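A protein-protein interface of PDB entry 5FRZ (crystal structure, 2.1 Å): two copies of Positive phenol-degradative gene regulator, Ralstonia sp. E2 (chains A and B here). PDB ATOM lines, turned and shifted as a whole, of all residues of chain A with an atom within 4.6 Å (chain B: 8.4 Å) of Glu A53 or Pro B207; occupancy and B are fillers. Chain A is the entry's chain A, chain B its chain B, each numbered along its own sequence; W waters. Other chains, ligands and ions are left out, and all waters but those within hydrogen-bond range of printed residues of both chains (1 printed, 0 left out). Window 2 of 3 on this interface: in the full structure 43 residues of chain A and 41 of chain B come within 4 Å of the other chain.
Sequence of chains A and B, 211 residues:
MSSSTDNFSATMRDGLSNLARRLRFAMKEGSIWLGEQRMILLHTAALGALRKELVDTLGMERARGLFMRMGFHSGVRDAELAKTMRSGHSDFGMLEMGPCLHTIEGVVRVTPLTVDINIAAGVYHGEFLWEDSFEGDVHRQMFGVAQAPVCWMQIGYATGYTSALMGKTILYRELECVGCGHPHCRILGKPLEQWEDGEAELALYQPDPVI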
ATOM      1  N   ALA A  49     -18.908 -12.504  25.576  1.00  0.00           N
ATOM      2  CA  ALA A  49     -17.967 -11.951  24.608  1.00  0.00           C
ATOM      3  C   ALA A  49     -18.631 -10.934  23.685  1.00  0.00           C
ATOM      4  O   ALA A  49     -18.096  -9.851  23.458  1.00  0.00           O
ATOM      5  CB  ALA A  49     -17.361 -13.043  23.800  1.00  0.00           C
ATOM      6  N   LEU A  50     -19.794 -11.283  23.145  1.00  0.00           N
ATOM      7  CA  LEU A  50     -20.543 -10.336  22.335  1.00  0.00           C
ATOM      8  C   LEU A  50     -20.860  -9.085  23.153  1.00  0.00           C
ATOM      9  O   LEU A  50     -20.669  -7.971  22.671  1.00  0.00           O
ATOM     10  CB  LEU A  50     -21.832 -10.955  21.812  1.00  0.00           C
ATOM     11  CG  LEU A  50     -22.683  -9.956  21.039  1.00  0.00           C
ATOM     12  CD1 LEU A  50     -22.084  -9.721  19.652  1.00  0.00           C
ATOM     13  CD2 LEU A  50     -24.145 -10.420  20.961  1.00  0.00           C
ATOM     14  N   ARG A  51     -21.300  -9.273  24.400  1.00  0.00           N
ATOM     15  CA  ARG A  51     -21.648  -8.129  25.247  1.00  0.00           C
ATOM     16  C   ARG A  51     -20.461  -7.193  25.421  1.00  0.00           C
ATOM     17  O   ARG A  51     -20.613  -5.971  25.398  1.00  0.00           O
ATOM     18  CB  ARG A  51     -22.138  -8.562  26.634  1.00  0.00           C
ATOM     19  CG  ARG A  51     -22.209  -7.362  27.606  1.00  0.00           C
ATOM     20  CD  ARG A  51     -22.549  -7.753  29.028  1.00  0.00           C
ATOM     21  NE  ARG A  51     -23.878  -8.304  29.007  1.00  0.00           N
ATOM     22  CZ  ARG A  51     -24.855  -7.989  29.840  1.00  0.00           C
ATOM     23  NH1 ARG A  51     -24.673  -7.134  30.835  1.00  0.00           N
ATOM     24  NH2 ARG A  51     -26.017  -8.566  29.661  1.00  0.00           N
ATOM     25  N   LYS A  52     -19.282  -7.785  25.602  1.00  0.00           N
ATOM     26  CA  LYS A  52     -18.051  -7.021  25.770  1.00  0.00           C
ATOM     27  C   LYS A  52     -17.699  -6.197  24.537  1.00  0.00           C
ATOM     28  O   LYS A  52     -17.331  -5.023  24.634  1.00  0.00           O
ATOM     29  CB  LYS A  52     -16.890  -7.949  26.118  1.00  0.00           C
ATOM     30  CG  LYS A  52     -15.576  -7.193  26.182  1.00  0.00           C
ATOM     31  CD  LYS A  52     -14.676  -7.703  27.283  1.00  0.00           C
ATOM     32  CE  LYS A  52     -13.427  -6.841  27.372  1.00  0.00           C
ATOM     33  NZ  LYS A  52     -13.794  -5.400  27.511  1.00  0.00           N
ATOM     34  N   GLU A  53     -17.823  -6.808  23.368  1.00  0.00           N
ATOM     35  CA  GLU A  53     -17.557  -6.099  22.124  1.00  0.00           C
ATOM     36  C   GLU A  53     -18.547  -4.959  21.865  1.00  0.00           C
ATOM     37  O   GLU A  53     -18.184  -3.938  21.268  1.00  0.00           O
ATOM     38  CB  GLU A  53     -17.579  -7.071  20.946  1.00  0.00           C
ATOM     39  CG  GLU A  53     -16.364  -7.980  20.851  1.00  0.00           C
ATOM     40  CD  GLU A  53     -16.097  -8.403  19.419  1.00  0.00           C
ATOM     41  OE1 GLU A  53     -15.769  -7.525  18.595  1.00  0.00           O
ATOM     42  OE2 GLU A  53     -16.231  -9.605  19.108  1.00  0.00           O
ATOM     43  N   LEU A  54     -19.794  -5.132  22.299  1.00  0.00           N
ATOM     44  CA  LEU A  54     -20.819  -4.115  22.064  1.00  0.00           C
ATOM     45  C   LEU A  54     -20.596  -2.897  22.967  1.00  0.00           C
ATOM     46  O   LEU A  54     -20.794  -1.755  22.546  1.00  0.00           O
ATOM     47  CB  LEU A  54     -22.226  -4.699  22.271  1.00  0.00           C
ATOM     48  CG  LEU A  54     -22.688  -5.705  21.208  1.00  0.00           C
ATOM     49  CD1 LEU A  54     -24.143  -6.116  21.384  1.00  0.00           C
ATOM     50  CD2 LEU A  54     -22.479  -5.139  19.810  1.00  0.00           C
ATOM     51  N   VAL A  55     -20.170  -3.148  24.201  1.00  0.00           N
ATOM     52  CA  VAL A  55     -19.872  -2.059  25.122  1.00  0.00           C
ATOM     53  C   VAL A  55     -18.657  -1.283  24.626  1.00  0.00           C
ATOM     54  O   VAL A  55     -18.732  -0.079  24.408  1.00  0.00           O
ATOM     55  CB  VAL A  55     -19.619  -2.564  26.558  1.00  0.00           C
ATOM     56  CG1 VAL A  55     -19.129  -1.429  27.443  1.00  0.00           C
ATOM     57  CG2 VAL A  55     -20.889  -3.170  27.135  1.00  0.00           C
ATOM     58  N   ASP A  56     -17.547  -1.988  24.427  1.00  0.00           N
ATOM     59  CA  ASP A  56     -16.318  -1.385  23.909  1.00  0.00           C
ATOM     60  C   ASP A  56     -16.529  -0.605  22.607  1.00  0.00           C
ATOM     61  O   ASP A  56     -15.875   0.400  22.366  1.00  0.00           O
ATOM     62  CB  ASP A  56     -15.260  -2.471  23.711  1.00  0.00           C
ATOM     63  CG  ASP A  56     -14.852  -3.119  25.017  1.00  0.00           C
ATOM     64  OD1 ASP A  56     -15.118  -2.516  26.081  1.00  0.00           O
ATOM     65  OD2 ASP A  56     -14.267  -4.224  24.992  1.00  0.00           O
ATOM     66  N   THR A  57     -17.469  -1.039  21.781  1.00  0.00           N
ATOM     67  CA  THR A  57     -17.656  -0.405  20.483  1.00  0.00           C
ATOM     68  C   THR A  57     -18.745   0.672  20.488  1.00  0.00           C
ATOM     69  O   THR A  57     -18.612   1.707  19.826  1.00  0.00           O
ATOM     70  CB  THR A  57     -17.980  -1.470  19.415  1.00  0.00           C
ATOM     71  OG1 THR A  57     -16.811  -2.273  19.200  1.00  0.00           O
ATOM     72  CG2 THR A  57     -18.368  -0.835  18.112  1.00  0.00           C
ATOM     73  N   LEU B  58     -24.545  -1.083  12.078  1.00  0.00           N
ATOM     74  CA  LEU B  58     -23.093  -1.207  11.948  1.00  0.00           C
ATOM     75  C   LEU B  58     -22.732  -1.678  10.551  1.00  0.00           C
ATOM     76  O   LEU B  58     -21.590  -1.558  10.119  1.00  0.00           O
ATOM     77  CB  LEU B  58     -22.522  -2.169  12.995  1.00  0.00           C
ATOM     78  CG  LEU B  58     -22.962  -2.008  14.456  1.00  0.00           C
ATOM     79  CD1 LEU B  58     -22.270  -3.029  15.346  1.00  0.00           C
ATOM     80  CD2 LEU B  58     -22.697  -0.615  14.962  1.00  0.00           C
ATOM     81  N   ARG B  62     -19.576  -5.579   9.528  1.00  0.00           N
ATOM     82  CA  ARG B  62     -19.289  -5.460  10.953  1.00  0.00           C
ATOM     83  C   ARG B  62     -20.127  -6.432  11.787  1.00  0.00           C
ATOM     84  O   ARG B  62     -19.666  -6.945  12.803  1.00  0.00           O
ATOM     85  CB  ARG B  62     -19.537  -4.021  11.420  1.00  0.00           C
ATOM     86  CG  ARG B  62     -18.280  -3.266  11.741  1.00  0.00           C
ATOM     87  CD  ARG B  62     -17.639  -3.858  12.977  1.00  0.00           C
ATOM     88  NE  ARG B  62     -16.350  -3.246  13.272  1.00  0.00           N
ATOM     89  CZ  ARG B  62     -15.704  -3.391  14.423  1.00  0.00           C
ATOM     90  NH1 ARG B  62     -16.239  -4.122  15.397  1.00  0.00           N
ATOM     91  NH2 ARG B  62     -14.529  -2.799  14.605  1.00  0.00           N
ATOM     92  N   GLY B  65     -18.884 -10.165  11.544  1.00  0.00           N
ATOM     93  CA  GLY B  65     -17.733 -10.423  12.384  1.00  0.00           C
ATOM     94  C   GLY B  65     -18.046 -10.628  13.854  1.00  0.00           C
ATOM     95  O   GLY B  65     -17.504 -11.540  14.471  1.00  0.00           O
ATOM     96  N   LEU B  66     -18.881  -9.759  14.427  1.00  0.00           N
ATOM     97  CA  LEU B  66     -19.361  -9.947  15.792  1.00  0.00           C
ATOM     98  C   LEU B  66     -19.881 -11.365  16.002  1.00  0.00           C
ATOM     99  O   LEU B  66     -19.515 -12.047  16.954  1.00  0.00           O
ATOM    100  CB  LEU B  66     -20.474  -8.950  16.111  1.00  0.00           C
ATOM    101  CG  LEU B  66     -20.030  -7.498  16.256  1.00  0.00           C
ATOM    102  CD1 LEU B  66     -21.218  -6.568  16.454  1.00  0.00           C
ATOM    103  CD2 LEU B  66     -19.074  -7.405  17.422  1.00  0.00           C
ATOM    104  N   PHE B  67     -20.748 -11.801  15.097  1.00  0.00           N
ATOM    105  CA  PHE B  67     -21.356 -13.105  15.227  1.00  0.00           C
ATOM    106  C   PHE B  67     -20.352 -14.224  15.010  1.00  0.00           C
ATOM    107  O   PHE B  67     -20.386 -15.213  15.732  1.00  0.00           O
ATOM    108  CB  PHE B  67     -22.534 -13.230  14.274  1.00  0.00           C
ATOM    109  CG  PHE B  67     -23.794 -12.638  14.824  1.00  0.00           C
ATOM    110  CD1 PHE B  67     -24.544 -13.330  15.756  1.00  0.00           C
ATOM    111  CD2 PHE B  67     -24.214 -11.368  14.440  1.00  0.00           C
ATOM    112  CE1 PHE B  67     -25.719 -12.769  16.289  1.00  0.00           C
ATOM    113  CE2 PHE B  67     -25.383 -10.806  14.963  1.00  0.00           C
ATOM    114  CZ  PHE B  67     -26.127 -11.505  15.890  1.00  0.00           C
ATOM    115  N   MET B  68     -19.454 -14.073  14.038  1.00  0.00           N
ATOM    116  CA  MET B  68     -18.447 -15.108  13.817  1.00  0.00           C
ATOM    117  C   MET B  68     -17.599 -15.319  15.071  1.00  0.00           C
ATOM    118  O   MET B  68     -17.204 -16.452  15.372  1.00  0.00           O
ATOM    119  CB  MET B  68     -17.530 -14.760  12.637  1.00  0.00           C
ATOM    120  CG  MET B  68     -18.148 -14.926  11.272  1.00  0.00           C
ATOM    121  SD  MET B  68     -17.097 -14.274   9.954  1.00  0.00           S
ATOM    122  CE  MET B  68     -15.658 -15.320  10.097  1.00  0.00           C
ATOM    123  N   ARG B  69     -17.319 -14.235  15.802  1.00  0.00           N
ATOM    124  CA  ARG B  69     -16.440 -14.328  16.980  1.00  0.00           C
ATOM    125  C   ARG B  69     -17.207 -14.875  18.180  1.00  0.00           C
ATOM    126  O   ARG B  69     -16.658 -15.625  19.003  1.00  0.00           O
ATOM    127  CB  ARG B  69     -15.803 -12.968  17.305  1.00  0.00           C
ATOM    128  CG  ARG B  69     -14.818 -12.477  16.229  1.00  0.00           C
ATOM    129  CD  ARG B  69     -14.125 -11.183  16.644  1.00  0.00           C
ATOM    130  NE  ARG B  69     -15.047 -10.060  16.729  1.00  0.00           N
ATOM    131  CZ  ARG B  69     -15.279  -9.203  15.734  1.00  0.00           C
ATOM    132  NH1 ARG B  69     -14.652  -9.335  14.573  1.00  0.00           N
ATOM    133  NH2 ARG B  69     -16.138  -8.206  15.896  1.00  0.00           N
ATOM    134  N   MET B  70     -18.491 -14.538  18.259  1.00  0.00           N
ATOM    135  CA  MET B  70     -19.379 -15.203  19.206  1.00  0.00           C
ATOM    136  C   MET B  70     -19.429 -16.717  18.943  1.00  0.00           C
ATOM    137  O   MET B  70     -19.264 -17.528  19.851  1.00  0.00           O
ATOM    138  CB  MET B  70     -20.782 -14.599  19.133  1.00  0.00           C
ATOM    139  CG  MET B  70     -21.615 -14.821  20.386  1.00  0.00           C
ATOM    140  SD  MET B  70     -23.358 -14.400  20.130  1.00  0.00           S
ATOM    141  CE  MET B  70     -23.203 -13.076  18.955  1.00  0.00           C
ATOM    142  N   GLY B  71     -19.648 -17.093  17.696  1.00  0.00           N
ATOM    143  CA  GLY B  71     -19.626 -18.494  17.331  1.00  0.00           C
ATOM    144  C   GLY B  71     -18.277 -19.106  17.683  1.00  0.00           C
ATOM    145  O   GLY B  71     -18.205 -20.208  18.217  1.00  0.00           O
ATOM    146  N   HIS B  73     -16.318 -18.416  20.178  1.00  0.00           N
ATOM    147  CA  HIS B  73     -16.044 -18.803  21.571  1.00  0.00           C
ATOM    148  C   HIS B  73     -16.883 -19.988  21.993  1.00  0.00           C
ATOM    149  O   HIS B  73     -16.424 -20.777  22.822  1.00  0.00           O
ATOM    150  CB  HIS B  73     -16.215 -17.688  22.626  1.00  0.00           C
ATOM    151  CG  HIS B  73     -15.429 -16.469  22.342  1.00  0.00           C
ATOM    152  ND1 HIS B  73     -14.186 -16.520  21.729  1.00  0.00           N
ATOM    153  CD2 HIS B  73     -15.473 -15.276  22.990  1.00  0.00           C
ATOM    154  CE1 HIS B  73     -13.662 -15.310  21.734  1.00  0.00           C
ATOM    155  NE2 HIS B  73     -14.420 -14.534  22.536  1.00  0.00           N
ATOM    156  N   LEU B 202      -8.808 -14.834   8.572  1.00  0.00           N
ATOM    157  CA  LEU B 202      -8.350 -14.883   9.954  1.00  0.00           C
ATOM    158  C   LEU B 202      -8.611 -13.559  10.672  1.00  0.00           C
ATOM    159  O   LEU B 202      -8.862 -13.542  11.877  1.00  0.00           O
ATOM    160  CB  LEU B 202      -6.858 -15.222  10.021  1.00  0.00           C
ATOM    161  CG  LEU B 202      -6.241 -15.293  11.421  1.00  0.00           C
ATOM    162  CD1 LEU B 202      -6.928 -16.375  12.241  1.00  0.00           C
ATOM    163  CD2 LEU B 202      -4.755 -15.552  11.347  1.00  0.00           C
ATOM    164  N   ALA B 203      -8.547 -12.459   9.924  1.00  0.00           N
ATOM    165  CA  ALA B 203      -8.762 -11.121  10.472  1.00  0.00           C
ATOM    166  C   ALA B 203     -10.129 -10.971  11.138  1.00  0.00           C
ATOM    167  O   ALA B 203     -10.250 -10.342  12.189  1.00  0.00           O
ATOM    168  CB  ALA B 203      -8.604 -10.076   9.380  1.00  0.00           C
ATOM    169  N   LEU B 204     -11.153 -11.559  10.533  1.00  0.00           N
ATOM    170  CA  LEU B 204     -12.519 -11.430  11.038  1.00  0.00           C
ATOM    171  C   LEU B 204     -12.687 -11.932  12.472  1.00  0.00           C
ATOM    172  O   LEU B 204     -13.697 -11.648  13.120  1.00  0.00           O
ATOM    173  CB  LEU B 204     -13.475 -12.186  10.127  1.00  0.00           C
ATOM    174  CG  LEU B 204     -13.413 -11.771   8.661  1.00  0.00           C
ATOM    175  CD1 LEU B 204     -14.022 -12.848   7.799  1.00  0.00           C
ATOM    176  CD2 LEU B 204     -14.157 -10.466   8.475  1.00  0.00           C
ATOM    177  N   TYR B 205     -11.700 -12.674  12.960  1.00  0.00           N
ATOM    178  CA  TYR B 205     -11.785 -13.310  14.269  1.00  0.00           C
ATOM    179  C   TYR B 205     -11.092 -12.479  15.330  1.00  0.00           C
ATOM    180  O   TYR B 205     -10.929 -12.913  16.476  1.00  0.00           O
ATOM    181  CB  TYR B 205     -11.200 -14.725  14.216  1.00  0.00           C
ATOM    182  CG  TYR B 205     -12.109 -15.676  13.474  1.00  0.00           C
ATOM    183  CD1 TYR B 205     -13.274 -16.160  14.070  1.00  0.00           C
ATOM    184  CD2 TYR B 205     -11.835 -16.052  12.175  1.00  0.00           C
ATOM    185  CE1 TYR B 205     -14.128 -17.018  13.394  1.00  0.00           C
ATOM    186  CE2 TYR B 205     -12.684 -16.910  11.488  1.00  0.00           C
ATOM    187  CZ  TYR B 205     -13.833 -17.387  12.106  1.00  0.00           C
ATOM    188  OH  TYR B 205     -14.679 -18.237  11.427  1.00  0.00           O
ATOM    189  N   GLN B 206     -10.690 -11.277  14.938  1.00  0.00           N
ATOM    190  CA  GLN B 206     -10.110 -10.327  15.869  1.00  0.00           C
ATOM    191  C   GLN B 206     -11.087  -9.186  16.109  1.00  0.00           C
ATOM    192  O   GLN B 206     -11.672  -8.670  15.162  1.00  0.00           O
ATOM    193  CB  GLN B 206      -8.771  -9.806  15.348  1.00  0.00           C
ATOM    194  CG  GLN B 206      -7.621 -10.789  15.558  1.00  0.00           C
ATOM    195  CD  GLN B 206      -7.363 -11.068  17.033  1.00  0.00           C
ATOM    196  OE1 GLN B 206      -7.767 -12.105  17.565  1.00  0.00           O
ATOM    197  NE2 GLN B 206      -6.702 -10.129  17.705  1.00  0.00           N
ATOM    198  N   PRO B 207     -11.302  -8.838  17.390  1.00  0.00           N
ATOM    199  CA  PRO B 207     -12.215  -7.789  17.883  1.00  0.00           C
ATOM    200  C   PRO B 207     -12.200  -6.487  17.078  1.00  0.00           C
ATOM    201  O   PRO B 207     -11.231  -6.208  16.374  1.00  0.00           O
ATOM    202  CB  PRO B 207     -11.710  -7.536  19.305  1.00  0.00           C
ATOM    203  CG  PRO B 207     -11.028  -8.850  19.719  1.00  0.00           C
ATOM    204  CD  PRO B 207     -10.838  -9.706  18.488  1.00  0.00           C
HETATM  205  O   HOH W   1     -18.636 -10.989  19.242  1.00  0.00           O
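The side-chain carboxylate (OE2) of Glu A53 lies within salt-bridge range of the guanidinium group (NE) of Arg B69, at 2.7 Å.
OG1 of Thr A57 sits at hydrogen-bond distance from O of Glu A53 (3.0 Å).
The guanidinium group (NH1) of Arg B69 sits at hydrogen-bond distance from the backbone carbonyl oxygen (O) of Leu B204.
The backbone carbonyl oxygen (O) of Gln B206 is in hydrogen-bond range of the guanidinium group (NH1) of Arg B69 (3.1 Å).
Ala A49 touches His B73 (CB to CD2, 3.0 Å).
Leu A50 touches Leu B66 (CD1 to CB, 3.97 Å).
CE of Met B70 touches CD2 of Leu A50, 3.5 Å away.
Glu A53 touches Leu B66 (OE1 to CD2, 3.5 Å).
CA of Pro B207 touches OE1 of Glu A53 (3.6 Å).
Leu A54 touches Leu B66.
Of the printed residues of chain B, Leu A50 touches Leu B66 (3.97 Å) and Met B70 (3.5 Å).
Glu A53 touches just these residues of chain B: Leu B66, Arg B69 and Pro B207.
Printed residues of chain B within 4 Å of Leu A54: Leu B66.
Of the printed residues of chain A, Arg B69 touches Glu A53 (2.7 Å).
Of the printed residues of chain A, Met B70 touches Leu A50.
Pro B207 touches just one residue of chain A: Glu A53 (3.6 Å).
The nearest residue of chain B that does not touch Glu A53 is Arg B62 (4.7 Å).
Printed residues of chain A that touch a printed residue of chain B: Ala A49, Leu A50, Glu A53 and Leu A54.
Among the printed residues, 7 pairs touch across the chains.
Among the printed residues, Asp or Glu carboxylates within 4 Å of a Lys or Arg side-chain nitrogen of the other chain: Glu A53 with Arg B69 (2.7 Å).
No position is printed for both chains.
Water W1 lies within hydrogen-bond range of the backbone carbonyl oxygen of Leu B66 (2.7 Å) and the side-chain carboxylate of Glu A53 (2.8 Å).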
